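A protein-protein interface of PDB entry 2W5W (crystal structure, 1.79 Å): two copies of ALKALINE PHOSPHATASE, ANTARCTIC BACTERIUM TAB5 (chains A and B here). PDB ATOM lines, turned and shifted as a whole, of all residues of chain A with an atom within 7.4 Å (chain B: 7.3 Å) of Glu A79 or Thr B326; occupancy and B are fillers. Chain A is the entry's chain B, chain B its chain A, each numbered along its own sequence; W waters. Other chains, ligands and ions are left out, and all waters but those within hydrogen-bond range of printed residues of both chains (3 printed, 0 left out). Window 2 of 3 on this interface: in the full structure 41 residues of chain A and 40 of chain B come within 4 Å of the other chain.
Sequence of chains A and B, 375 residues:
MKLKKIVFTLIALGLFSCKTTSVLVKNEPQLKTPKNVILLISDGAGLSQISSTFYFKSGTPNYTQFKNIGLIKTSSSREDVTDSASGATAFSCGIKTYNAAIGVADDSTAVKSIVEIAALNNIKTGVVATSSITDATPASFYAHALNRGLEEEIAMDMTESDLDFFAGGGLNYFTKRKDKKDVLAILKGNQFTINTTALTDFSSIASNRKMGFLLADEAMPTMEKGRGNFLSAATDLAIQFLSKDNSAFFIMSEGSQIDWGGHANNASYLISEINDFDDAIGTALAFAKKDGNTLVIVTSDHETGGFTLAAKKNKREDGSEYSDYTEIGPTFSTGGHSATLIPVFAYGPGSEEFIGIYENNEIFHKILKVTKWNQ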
ATOM      1  N   THR A  74     -32.306 -24.278   8.430  1.00  0.00           N
ATOM      2  CA  THR A  74     -32.391 -25.402   7.499  1.00  0.00           C
ATOM      3  C   THR A  74     -31.230 -25.522   6.517  1.00  0.00           C
ATOM      4  O   THR A  74     -31.250 -26.425   5.666  1.00  0.00           O
ATOM      5  CB  THR A  74     -33.697 -25.360   6.677  1.00  0.00           C
ATOM      6  OG1 THR A  74     -33.729 -24.134   5.919  1.00  0.00           O
ATOM      7  CG2 THR A  74     -34.905 -25.423   7.605  1.00  0.00           C
ATOM      8  N   SER A  75     -30.225 -24.650   6.607  1.00  0.00           N
ATOM      9  CA  SER A  75     -29.131 -24.711   5.621  1.00  0.00           C
ATOM     10  C   SER A  75     -28.424 -26.069   5.614  1.00  0.00           C
ATOM     11  O   SER A  75     -28.371 -26.763   6.628  1.00  0.00           O
ATOM     12  CB  SER A  75     -28.111 -23.573   5.830  1.00  0.00           C
ATOM     13  OG  SER A  75     -28.722 -22.309   5.611  1.00  0.00           O
ATOM     14  N   SER A  76     -27.902 -26.463   4.457  1.00  0.00           N
ATOM     15  CA  SER A  76     -27.213 -27.747   4.347  1.00  0.00           C
ATOM     16  C   SER A  76     -25.741 -27.558   4.695  1.00  0.00           C
ATOM     17  O   SER A  76     -25.345 -26.478   5.142  1.00  0.00           O
ATOM     18  CB  SER A  76     -27.361 -28.302   2.932  1.00  0.00           C
ATOM     19  OG  SER A  76     -26.480 -27.626   2.042  1.00  0.00           O
ATOM     20  N   SER A  77     -24.915 -28.584   4.480  1.00  0.00           N
ATOM     21  CA  SER A  77     -23.500 -28.444   4.800  1.00  0.00           C
ATOM     22  C   SER A  77     -22.785 -27.569   3.765  1.00  0.00           C
ATOM     23  O   SER A  77     -21.686 -27.080   4.014  1.00  0.00           O
ATOM     24  CB  SER A  77     -22.831 -29.819   4.860  1.00  0.00           C
ATOM     25  OG  SER A  77     -22.929 -30.468   3.597  1.00  0.00           O
ATOM     26  N   ARG A  78     -23.389 -27.396   2.594  1.00  0.00           N
ATOM     27  CA  ARG A  78     -22.718 -26.698   1.493  1.00  0.00           C
ATOM     28  C   ARG A  78     -23.517 -25.524   0.915  1.00  0.00           C
ATOM     29  O   ARG A  78     -22.977 -24.737   0.132  1.00  0.00           O
ATOM     30  CB  ARG A  78     -22.410 -27.666   0.351  1.00  0.00           C
ATOM     31  CG  ARG A  78     -21.501 -28.823   0.742  1.00  0.00           C
ATOM     32  CD  ARG A  78     -20.978 -29.545  -0.486  1.00  0.00           C
ATOM     33  NE  ARG A  78     -20.300 -30.768  -0.072  1.00  0.00           N
ATOM     34  CZ  ARG A  78     -19.861 -31.706  -0.902  1.00  0.00           C
ATOM     35  NH1 ARG A  78     -20.024 -31.568  -2.212  1.00  0.00           N
ATOM     36  NH2 ARG A  78     -19.263 -32.785  -0.416  1.00  0.00           N
ATOM     37  N   GLU A  79     -24.795 -25.415   1.269  1.00  0.00           N
ATOM     38  CA  GLU A  79     -25.678 -24.476   0.581  1.00  0.00           C
ATOM     39  C   GLU A  79     -26.556 -23.740   1.579  1.00  0.00           C
ATOM     40  O   GLU A  79     -27.137 -24.362   2.467  1.00  0.00           O
ATOM     41  CB  GLU A  79     -26.592 -25.225  -0.410  1.00  0.00           C
ATOM     42  CG  GLU A  79     -25.892 -25.806  -1.656  1.00  0.00           C
ATOM     43  CD  GLU A  79     -25.575 -27.302  -1.566  1.00  0.00           C
ATOM     44  OE1 GLU A  79     -25.899 -27.948  -0.538  1.00  0.00           O
ATOM     45  OE2 GLU A  79     -24.977 -27.847  -2.533  1.00  0.00           O
ATOM     46  N   ASP A  80     -26.678 -22.425   1.425  1.00  0.00           N
ATOM     47  CA  ASP A  80     -27.558 -21.663   2.310  1.00  0.00           C
ATOM     48  C   ASP A  80     -29.022 -22.092   2.164  1.00  0.00           C
ATOM     49  O   ASP A  80     -29.782 -22.097   3.132  1.00  0.00           O
ATOM     50  CB  ASP A  80     -27.425 -20.160   2.031  1.00  0.00           C
ATOM     51  CG  ASP A  80     -26.194 -19.543   2.689  1.00  0.00           C
ATOM     52  OD1 ASP A  80     -25.616 -20.171   3.592  1.00  0.00           O
ATOM     53  OD2 ASP A  80     -25.821 -18.416   2.314  1.00  0.00           O
ATOM     54  N   VAL A  81     -29.431 -22.417   0.939  1.00  0.00           N
ATOM     55  CA  VAL A  81     -30.804 -22.844   0.698  1.00  0.00           C
ATOM     56  C   VAL A  81     -30.803 -24.342   0.512  1.00  0.00           C
ATOM     57  O   VAL A  81     -30.162 -24.861  -0.405  1.00  0.00           O
ATOM     58  CB  VAL A  81     -31.414 -22.187  -0.557  1.00  0.00           C
ATOM     59  CG1 VAL A  81     -32.856 -22.714  -0.772  1.00  0.00           C
ATOM     60  CG2 VAL A  81     -31.418 -20.672  -0.402  1.00  0.00           C
ATOM     61  N   THR A  82     -31.522 -25.043   1.382  1.00  0.00           N
ATOM     62  CA  THR A  82     -31.462 -26.496   1.345  1.00  0.00           C
ATOM     63  C   THR A  82     -32.398 -27.098   0.289  1.00  0.00           C
ATOM     64  O   THR A  82     -33.327 -26.433  -0.180  1.00  0.00           O
ATOM     65  CB  THR A  82     -31.808 -27.092   2.725  1.00  0.00           C
ATOM     66  OG1 THR A  82     -31.514 -28.492   2.717  1.00  0.00           O
ATOM     67  CG2 THR A  82     -33.282 -26.891   3.030  1.00  0.00           C
ATOM     68  N   ASP A  83     -32.132 -28.342  -0.103  1.00  0.00           N
ATOM     69  CA  ASP A  83     -33.115 -29.130  -0.851  1.00  0.00           C
ATOM     70  C   ASP A  83     -33.758 -30.154   0.083  1.00  0.00           C
ATOM     71  O   ASP A  83     -33.403 -30.238   1.257  1.00  0.00           O
ATOM     72  CB  ASP A  83     -32.506 -29.767  -2.111  1.00  0.00           C
ATOM     73  CG  ASP A  83     -31.855 -31.140  -1.864  1.00  0.00           C
ATOM     74  OD1 ASP A  83     -31.286 -31.384  -0.775  1.00  0.00           O
ATOM     75  OD2 ASP A  83     -31.899 -31.976  -2.799  1.00  0.00           O
ATOM     76  N   SER A  86     -31.142 -33.204   1.606  1.00  0.00           N
ATOM     77  CA  SER A  86     -30.317 -32.878   2.764  1.00  0.00           C
ATOM     78  C   SER A  86     -31.184 -32.456   3.966  1.00  0.00           C
ATOM     79  O   SER A  86     -30.859 -32.758   5.110  1.00  0.00           O
ATOM     80  CB  SER A  86     -29.313 -31.790   2.420  1.00  0.00           C
ATOM     81  OG  SER A  86     -29.984 -30.636   1.954  1.00  0.00           O
ATOM     82  N   THR A  97     -25.637 -32.274   5.623  1.00  0.00           N
ATOM     83  CA  THR A  97     -25.026 -32.921   4.465  1.00  0.00           C
ATOM     84  C   THR A  97     -25.335 -32.120   3.206  1.00  0.00           C
ATOM     85  O   THR A  97     -26.020 -31.110   3.283  1.00  0.00           O
ATOM     86  CB  THR A  97     -25.495 -34.387   4.345  1.00  0.00           C
ATOM     87  OG1 THR A  97     -24.715 -35.060   3.346  1.00  0.00           O
ATOM     88  CG2 THR A  97     -26.994 -34.463   4.001  1.00  0.00           C
ATOM     89  N   TYR A  98     -24.838 -32.566   2.051  1.00  0.00           N
ATOM     90  CA  TYR A  98     -24.958 -31.783   0.826  1.00  0.00           C
ATOM     91  C   TYR A  98     -26.338 -31.910   0.169  1.00  0.00           C
ATOM     92  O   TYR A  98     -27.000 -32.928   0.307  1.00  0.00           O
ATOM     93  CB  TYR A  98     -23.849 -32.150  -0.171  1.00  0.00           C
ATOM     94  CG  TYR A  98     -23.804 -33.619  -0.586  1.00  0.00           C
ATOM     95  CD1 TYR A  98     -24.569 -34.083  -1.650  1.00  0.00           C
ATOM     96  CD2 TYR A  98     -22.987 -34.527   0.079  1.00  0.00           C
ATOM     97  CE1 TYR A  98     -24.532 -35.427  -2.036  1.00  0.00           C
ATOM     98  CE2 TYR A  98     -22.933 -35.869  -0.299  1.00  0.00           C
ATOM     99  CZ  TYR A  98     -23.709 -36.309  -1.358  1.00  0.00           C
ATOM    100  OH  TYR A  98     -23.674 -37.631  -1.735  1.00  0.00           O
ATOM    101  N   ASN A  99     -26.777 -30.866  -0.527  1.00  0.00           N
ATOM    102  CA  ASN A  99     -28.049 -30.957  -1.245  1.00  0.00           C
ATOM    103  C   ASN A  99     -27.976 -32.141  -2.206  1.00  0.00           C
ATOM    104  O   ASN A  99     -26.974 -32.313  -2.895  1.00  0.00           O
ATOM    105  CB  ASN A  99     -28.343 -29.676  -2.030  1.00  0.00           C
ATOM    106  CG  ASN A  99     -28.825 -28.535  -1.131  1.00  0.00           C
ATOM    107  OD1 ASN A  99     -28.993 -28.712   0.070  1.00  0.00           O
ATOM    108  ND2 ASN A  99     -29.079 -27.377  -1.728  1.00  0.00           N
ATOM    109  N   ALA A 100     -29.046 -32.934  -2.220  1.00  0.00           N
ATOM    110  CA  ALA A 100     -29.172 -34.175  -2.993  1.00  0.00           C
ATOM    111  C   ALA A 100     -28.780 -35.447  -2.239  1.00  0.00           C
ATOM    112  O   ALA A 100     -29.105 -36.539  -2.676  1.00  0.00           O
ATOM    113  CB  ALA A 100     -28.445 -34.095  -4.341  1.00  0.00           C
ATOM    114  N   ASP A 106     -21.514 -35.645   4.468  1.00  0.00           N
ATOM    115  CA  ASP A 106     -20.936 -34.731   3.489  1.00  0.00           C
ATOM    116  C   ASP A 106     -19.922 -35.422   2.590  1.00  0.00           C
ATOM    117  O   ASP A 106     -19.772 -35.043   1.427  1.00  0.00           O
ATOM    118  CB  ASP A 106     -20.309 -33.522   4.183  1.00  0.00           C
ATOM    119  CG  ASP A 106     -19.971 -32.416   3.219  1.00  0.00           C
ATOM    120  OD1 ASP A 106     -20.906 -31.795   2.666  1.00  0.00           O
ATOM    121  OD2 ASP A 106     -18.767 -32.179   3.001  1.00  0.00           O
ATOM    122  N   ALA A 339     -34.588 -19.873   2.480  1.00  0.00           N
ATOM    123  CA  ALA A 339     -33.807 -20.207   3.670  1.00  0.00           C
ATOM    124  C   ALA A 339     -34.380 -19.708   5.000  1.00  0.00           C
ATOM    125  O   ALA A 339     -33.656 -19.673   5.997  1.00  0.00           O
ATOM    126  CB  ALA A 339     -32.381 -19.684   3.520  1.00  0.00           C
ATOM    127  N   TYR B  55     -28.324 -14.950   8.756  1.00  0.00           N
ATOM    128  CA  TYR B  55     -27.463 -15.004   7.573  1.00  0.00           C
ATOM    129  C   TYR B  55     -26.693 -13.720   7.302  1.00  0.00           C
ATOM    130  O   TYR B  55     -25.644 -13.757   6.659  1.00  0.00           O
ATOM    131  CB  TYR B  55     -28.266 -15.364   6.321  1.00  0.00           C
ATOM    132  CG  TYR B  55     -28.850 -16.741   6.404  1.00  0.00           C
ATOM    133  CD1 TYR B  55     -30.133 -16.940   6.895  1.00  0.00           C
ATOM    134  CD2 TYR B  55     -28.102 -17.850   6.037  1.00  0.00           C
ATOM    135  CE1 TYR B  55     -30.665 -18.208   7.009  1.00  0.00           C
ATOM    136  CE2 TYR B  55     -28.635 -19.125   6.130  1.00  0.00           C
ATOM    137  CZ  TYR B  55     -29.912 -19.292   6.619  1.00  0.00           C
ATOM    138  OH  TYR B  55     -30.439 -20.553   6.732  1.00  0.00           O
ATOM    139  N   ALA B 311     -33.086 -18.276  -3.198  1.00  0.00           N
ATOM    140  CA  ALA B 311     -31.784 -18.548  -3.787  1.00  0.00           C
ATOM    141  C   ALA B 311     -31.360 -17.426  -4.719  1.00  0.00           C
ATOM    142  O   ALA B 311     -32.181 -16.805  -5.388  1.00  0.00           O
ATOM    143  CB  ALA B 311     -31.814 -19.865  -4.545  1.00  0.00           C
ATOM    144  N   LYS B 312     -30.059 -17.171  -4.755  1.00  0.00           N
ATOM    145  CA  LYS B 312     -29.491 -16.221  -5.681  1.00  0.00           C
ATOM    146  C   LYS B 312     -29.924 -16.581  -7.105  1.00  0.00           C
ATOM    147  O   LYS B 312     -29.986 -17.758  -7.476  1.00  0.00           O
ATOM    148  CB  LYS B 312     -27.964 -16.251  -5.536  1.00  0.00           C
ATOM    149  CG  LYS B 312     -27.202 -15.317  -6.469  1.00  0.00           C
ATOM    150  CD  LYS B 312     -25.750 -15.203  -6.024  1.00  0.00           C
ATOM    151  CE  LYS B 312     -24.977 -14.207  -6.877  1.00  0.00           C
ATOM    152  NZ  LYS B 312     -24.601 -14.798  -8.187  1.00  0.00           N
ATOM    153  N   SER B 323     -31.292 -20.496 -10.737  1.00  0.00           N
ATOM    154  CA  SER B 323     -30.984 -20.348  -9.312  1.00  0.00           C
ATOM    155  C   SER B 323     -29.685 -21.023  -8.873  1.00  0.00           C
ATOM    156  O   SER B 323     -29.289 -22.056  -9.409  1.00  0.00           O
ATOM    157  CB  SER B 323     -32.141 -20.859  -8.454  1.00  0.00           C
ATOM    158  OG  SER B 323     -33.337 -20.180  -8.789  1.00  0.00           O
ATOM    159  N   ASP B 324     -29.028 -20.405  -7.897  1.00  0.00           N
ATOM    160  CA  ASP B 324     -27.867 -20.975  -7.236  1.00  0.00           C
ATOM    161  C   ASP B 324     -28.185 -21.070  -5.748  1.00  0.00           C
ATOM    162  O   ASP B 324     -28.166 -20.062  -5.040  1.00  0.00           O
ATOM    163  CB  ASP B 324     -26.654 -20.068  -7.441  1.00  0.00           C
ATOM    164  CG  ASP B 324     -25.417 -20.571  -6.724  1.00  0.00           C
ATOM    165  OD1 ASP B 324     -25.483 -21.626  -6.057  1.00  0.00           O
ATOM    166  OD2 ASP B 324     -24.369 -19.903  -6.835  1.00  0.00           O
ATOM    167  N   TYR B 325     -28.471 -22.280  -5.285  1.00  0.00           N
ATOM    168  CA  TYR B 325     -28.856 -22.505  -3.887  1.00  0.00           C
ATOM    169  C   TYR B 325     -27.730 -22.269  -2.892  1.00  0.00           C
ATOM    170  O   TYR B 325     -27.968 -22.244  -1.676  1.00  0.00           O
ATOM    171  CB  TYR B 325     -29.418 -23.918  -3.707  1.00  0.00           C
ATOM    172  CG  TYR B 325     -30.890 -24.056  -4.061  1.00  0.00           C
ATOM    173  CD1 TYR B 325     -31.476 -23.240  -5.023  1.00  0.00           C
ATOM    174  CD2 TYR B 325     -31.692 -25.006  -3.437  1.00  0.00           C
ATOM    175  CE1 TYR B 325     -32.817 -23.359  -5.349  1.00  0.00           C
ATOM    176  CE2 TYR B 325     -33.048 -25.129  -3.757  1.00  0.00           C
ATOM    177  CZ  TYR B 325     -33.603 -24.301  -4.712  1.00  0.00           C
ATOM    178  OH  TYR B 325     -34.952 -24.420  -5.046  1.00  0.00           O
ATOM    179  N   THR B 326     -26.506 -22.083  -3.375  1.00  0.00           N
ATOM    180  CA  THR B 326     -25.406 -21.879  -2.426  1.00  0.00           C
ATOM    181  C   THR B 326     -25.540 -20.555  -1.686  1.00  0.00           C
ATOM    182  O   THR B 326     -25.082 -20.422  -0.541  1.00  0.00           O
ATOM    183  CB  THR B 326     -24.014 -21.983  -3.084  1.00  0.00           C
ATOM    184  OG1 THR B 326     -23.899 -21.005  -4.121  1.00  0.00           O
ATOM    185  CG2 THR B 326     -23.829 -23.365  -3.687  1.00  0.00           C
ATOM    186  N   GLU B 327     -26.194 -19.585  -2.325  1.00  0.00           N
ATOM    187  CA  GLU B 327     -26.307 -18.236  -1.765  1.00  0.00           C
ATOM    188  C   GLU B 327     -27.728 -17.698  -1.776  1.00  0.00           C
ATOM    189  O   GLU B 327     -28.534 -18.097  -2.604  1.00  0.00           O
ATOM    190  CB  GLU B 327     -25.430 -17.257  -2.557  1.00  0.00           C
ATOM    191  CG  GLU B 327     -23.942 -17.524  -2.431  1.00  0.00           C
ATOM    192  CD  GLU B 327     -23.102 -16.449  -3.093  1.00  0.00           C
ATOM    193  OE1 GLU B 327     -22.125 -16.802  -3.786  1.00  0.00           O
ATOM    194  OE2 GLU B 327     -23.421 -15.252  -2.924  1.00  0.00           O
ATOM    195  N   ILE B 328     -27.999 -16.752  -0.874  1.00  0.00           N
ATOM    196  CA  ILE B 328     -29.303 -16.101  -0.770  1.00  0.00           C
ATOM    197  C   ILE B 328     -29.373 -14.775  -1.535  1.00  0.00           C
ATOM    198  O   ILE B 328     -28.464 -13.942  -1.450  1.00  0.00           O
ATOM    199  CB  ILE B 328     -29.642 -15.839   0.708  1.00  0.00           C
ATOM    200  CG1 ILE B 328     -29.809 -17.168   1.452  1.00  0.00           C
ATOM    201  CG2 ILE B 328     -30.870 -14.956   0.828  1.00  0.00           C
ATOM    202  CD1 ILE B 328     -29.788 -17.031   2.966  1.00  0.00           C
HETATM  203  O   HOH W   1     -22.840 -21.634   0.750  1.00  0.00           O
HETATM  204  O   HOH W   2     -32.916 -21.555   7.907  1.00  0.00           O
HETATM  205  O   HOH W   3     -25.662 -16.100   1.020  1.00  0.00           O
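The side-chain hydroxyl of Tyr B55 sits at hydrogen-bond distance from the side-chain hydroxyl of Ser A75 (2.7 Å).
O of Ala A339 sits at hydrogen-bond distance from OH of Tyr B55.
The backbone NH (N) of Asp A80 is in hydrogen-bond range of the backbone carbonyl oxygen (O) of Tyr B325.
The backbone carbonyl oxygen (O) of Tyr B325 is in hydrogen-bond range of the backbone NH (N) of Val A81, at 3.0 Å.
The backbone carbonyl oxygen (O) of Thr B326 lies within hydrogen-bond range of the backbone NH (N) of Asp A80 (3.2 Å).
The side-chain hydroxyl (OG1) of Thr B326 lies within hydrogen-bond range of the side-chain carboxylate (OD1) of Asp B324, 2.6 Å away.
The backbone carbonyl oxygen of Asp A80 sits at hydrogen-bond distance from the side-chain hydroxyl of Ser A75 (2.7 Å).
OG of Ser A76 lies close to OD1 of Asn A99 (3.4 Å).
O of Val A81 is in hydrogen-bond range of ND2 of Asn A99.
OG1 of Thr A82 is in hydrogen-bond range of OG of Ser A86, 2.7 Å away.
N of Asp A83 sits at hydrogen-bond distance from OD1 of Asn A99, 3.2 Å away.
Among the printed residues, merely in contact across the chains: Glu A79 with Tyr B325 (3.5 Å), Ala A339 with Ile B328 (3.8 Å), Glu A79 with Thr B326 (3.8 Å), Thr A82 with Tyr B325 (3.8 Å), Asp A80 with Ile B328 (3.9 Å), Asn A99 with Tyr B325 (3.9 Å) and Asp A80 with Tyr B55 (3.97 Å).
Glu A79 touches two residues of chain B.
Of the printed residues of chain B, Asp A80 touches Tyr B55 (3.97 Å), Tyr B325 (3.4 Å), Thr B326 (3.2 Å) and Ile B328 (3.9 Å).
Of the printed residues of chain B, Val A81 touches Tyr B325.
Of the printed residues of chain B, Thr A82 touches Tyr B325 (3.8 Å).
Printed residues of chain B within 4 Å of Asn A99: Tyr B325.
Of the printed residues of chain A, Tyr B325 touches Glu A79, Asp A80, Val A81, Thr A82 and Asn A99.
Of chain A, only Glu A79 and Asp A80 come within 4 Å of Thr B326.
Glu B327 touches none of the printed residues of chain A.
Of the 17 printed residues of chain A, 7 touch a printed residue of chain B.
Hydrophobic or aromatic side chains of chain A that line the printed part of chain B: Val A81 and Ala A339.
Of the 9 printed residues of chain B, 4 touch a printed residue of chain A.
Hydrophobic or aromatic side chains of chain B that line the printed part of chain A: Tyr B55, Tyr B325 and Ile B328.
Along chain B the printed residues that touch a printed residue of chain A span positions 55 to 328.
No position is printed for both chains.
Water W3 lies within hydrogen-bond range of the side-chain carboxylate of Asp A80 (2.7 Å) and the backbone NH of Ile B328 (3.1 Å).
Water W2 lies within hydrogen-bond range of O of Ala A339 (2.8 Å), N of Thr A74 (2.8 Å) and OH of Tyr B55 (2.9 Å).
Water W1 bridges the backbone carbonyl oxygen of Thr B326 (2.9 Å) and the backbone carbonyl oxygen of Arg A78 (3.2 Å).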
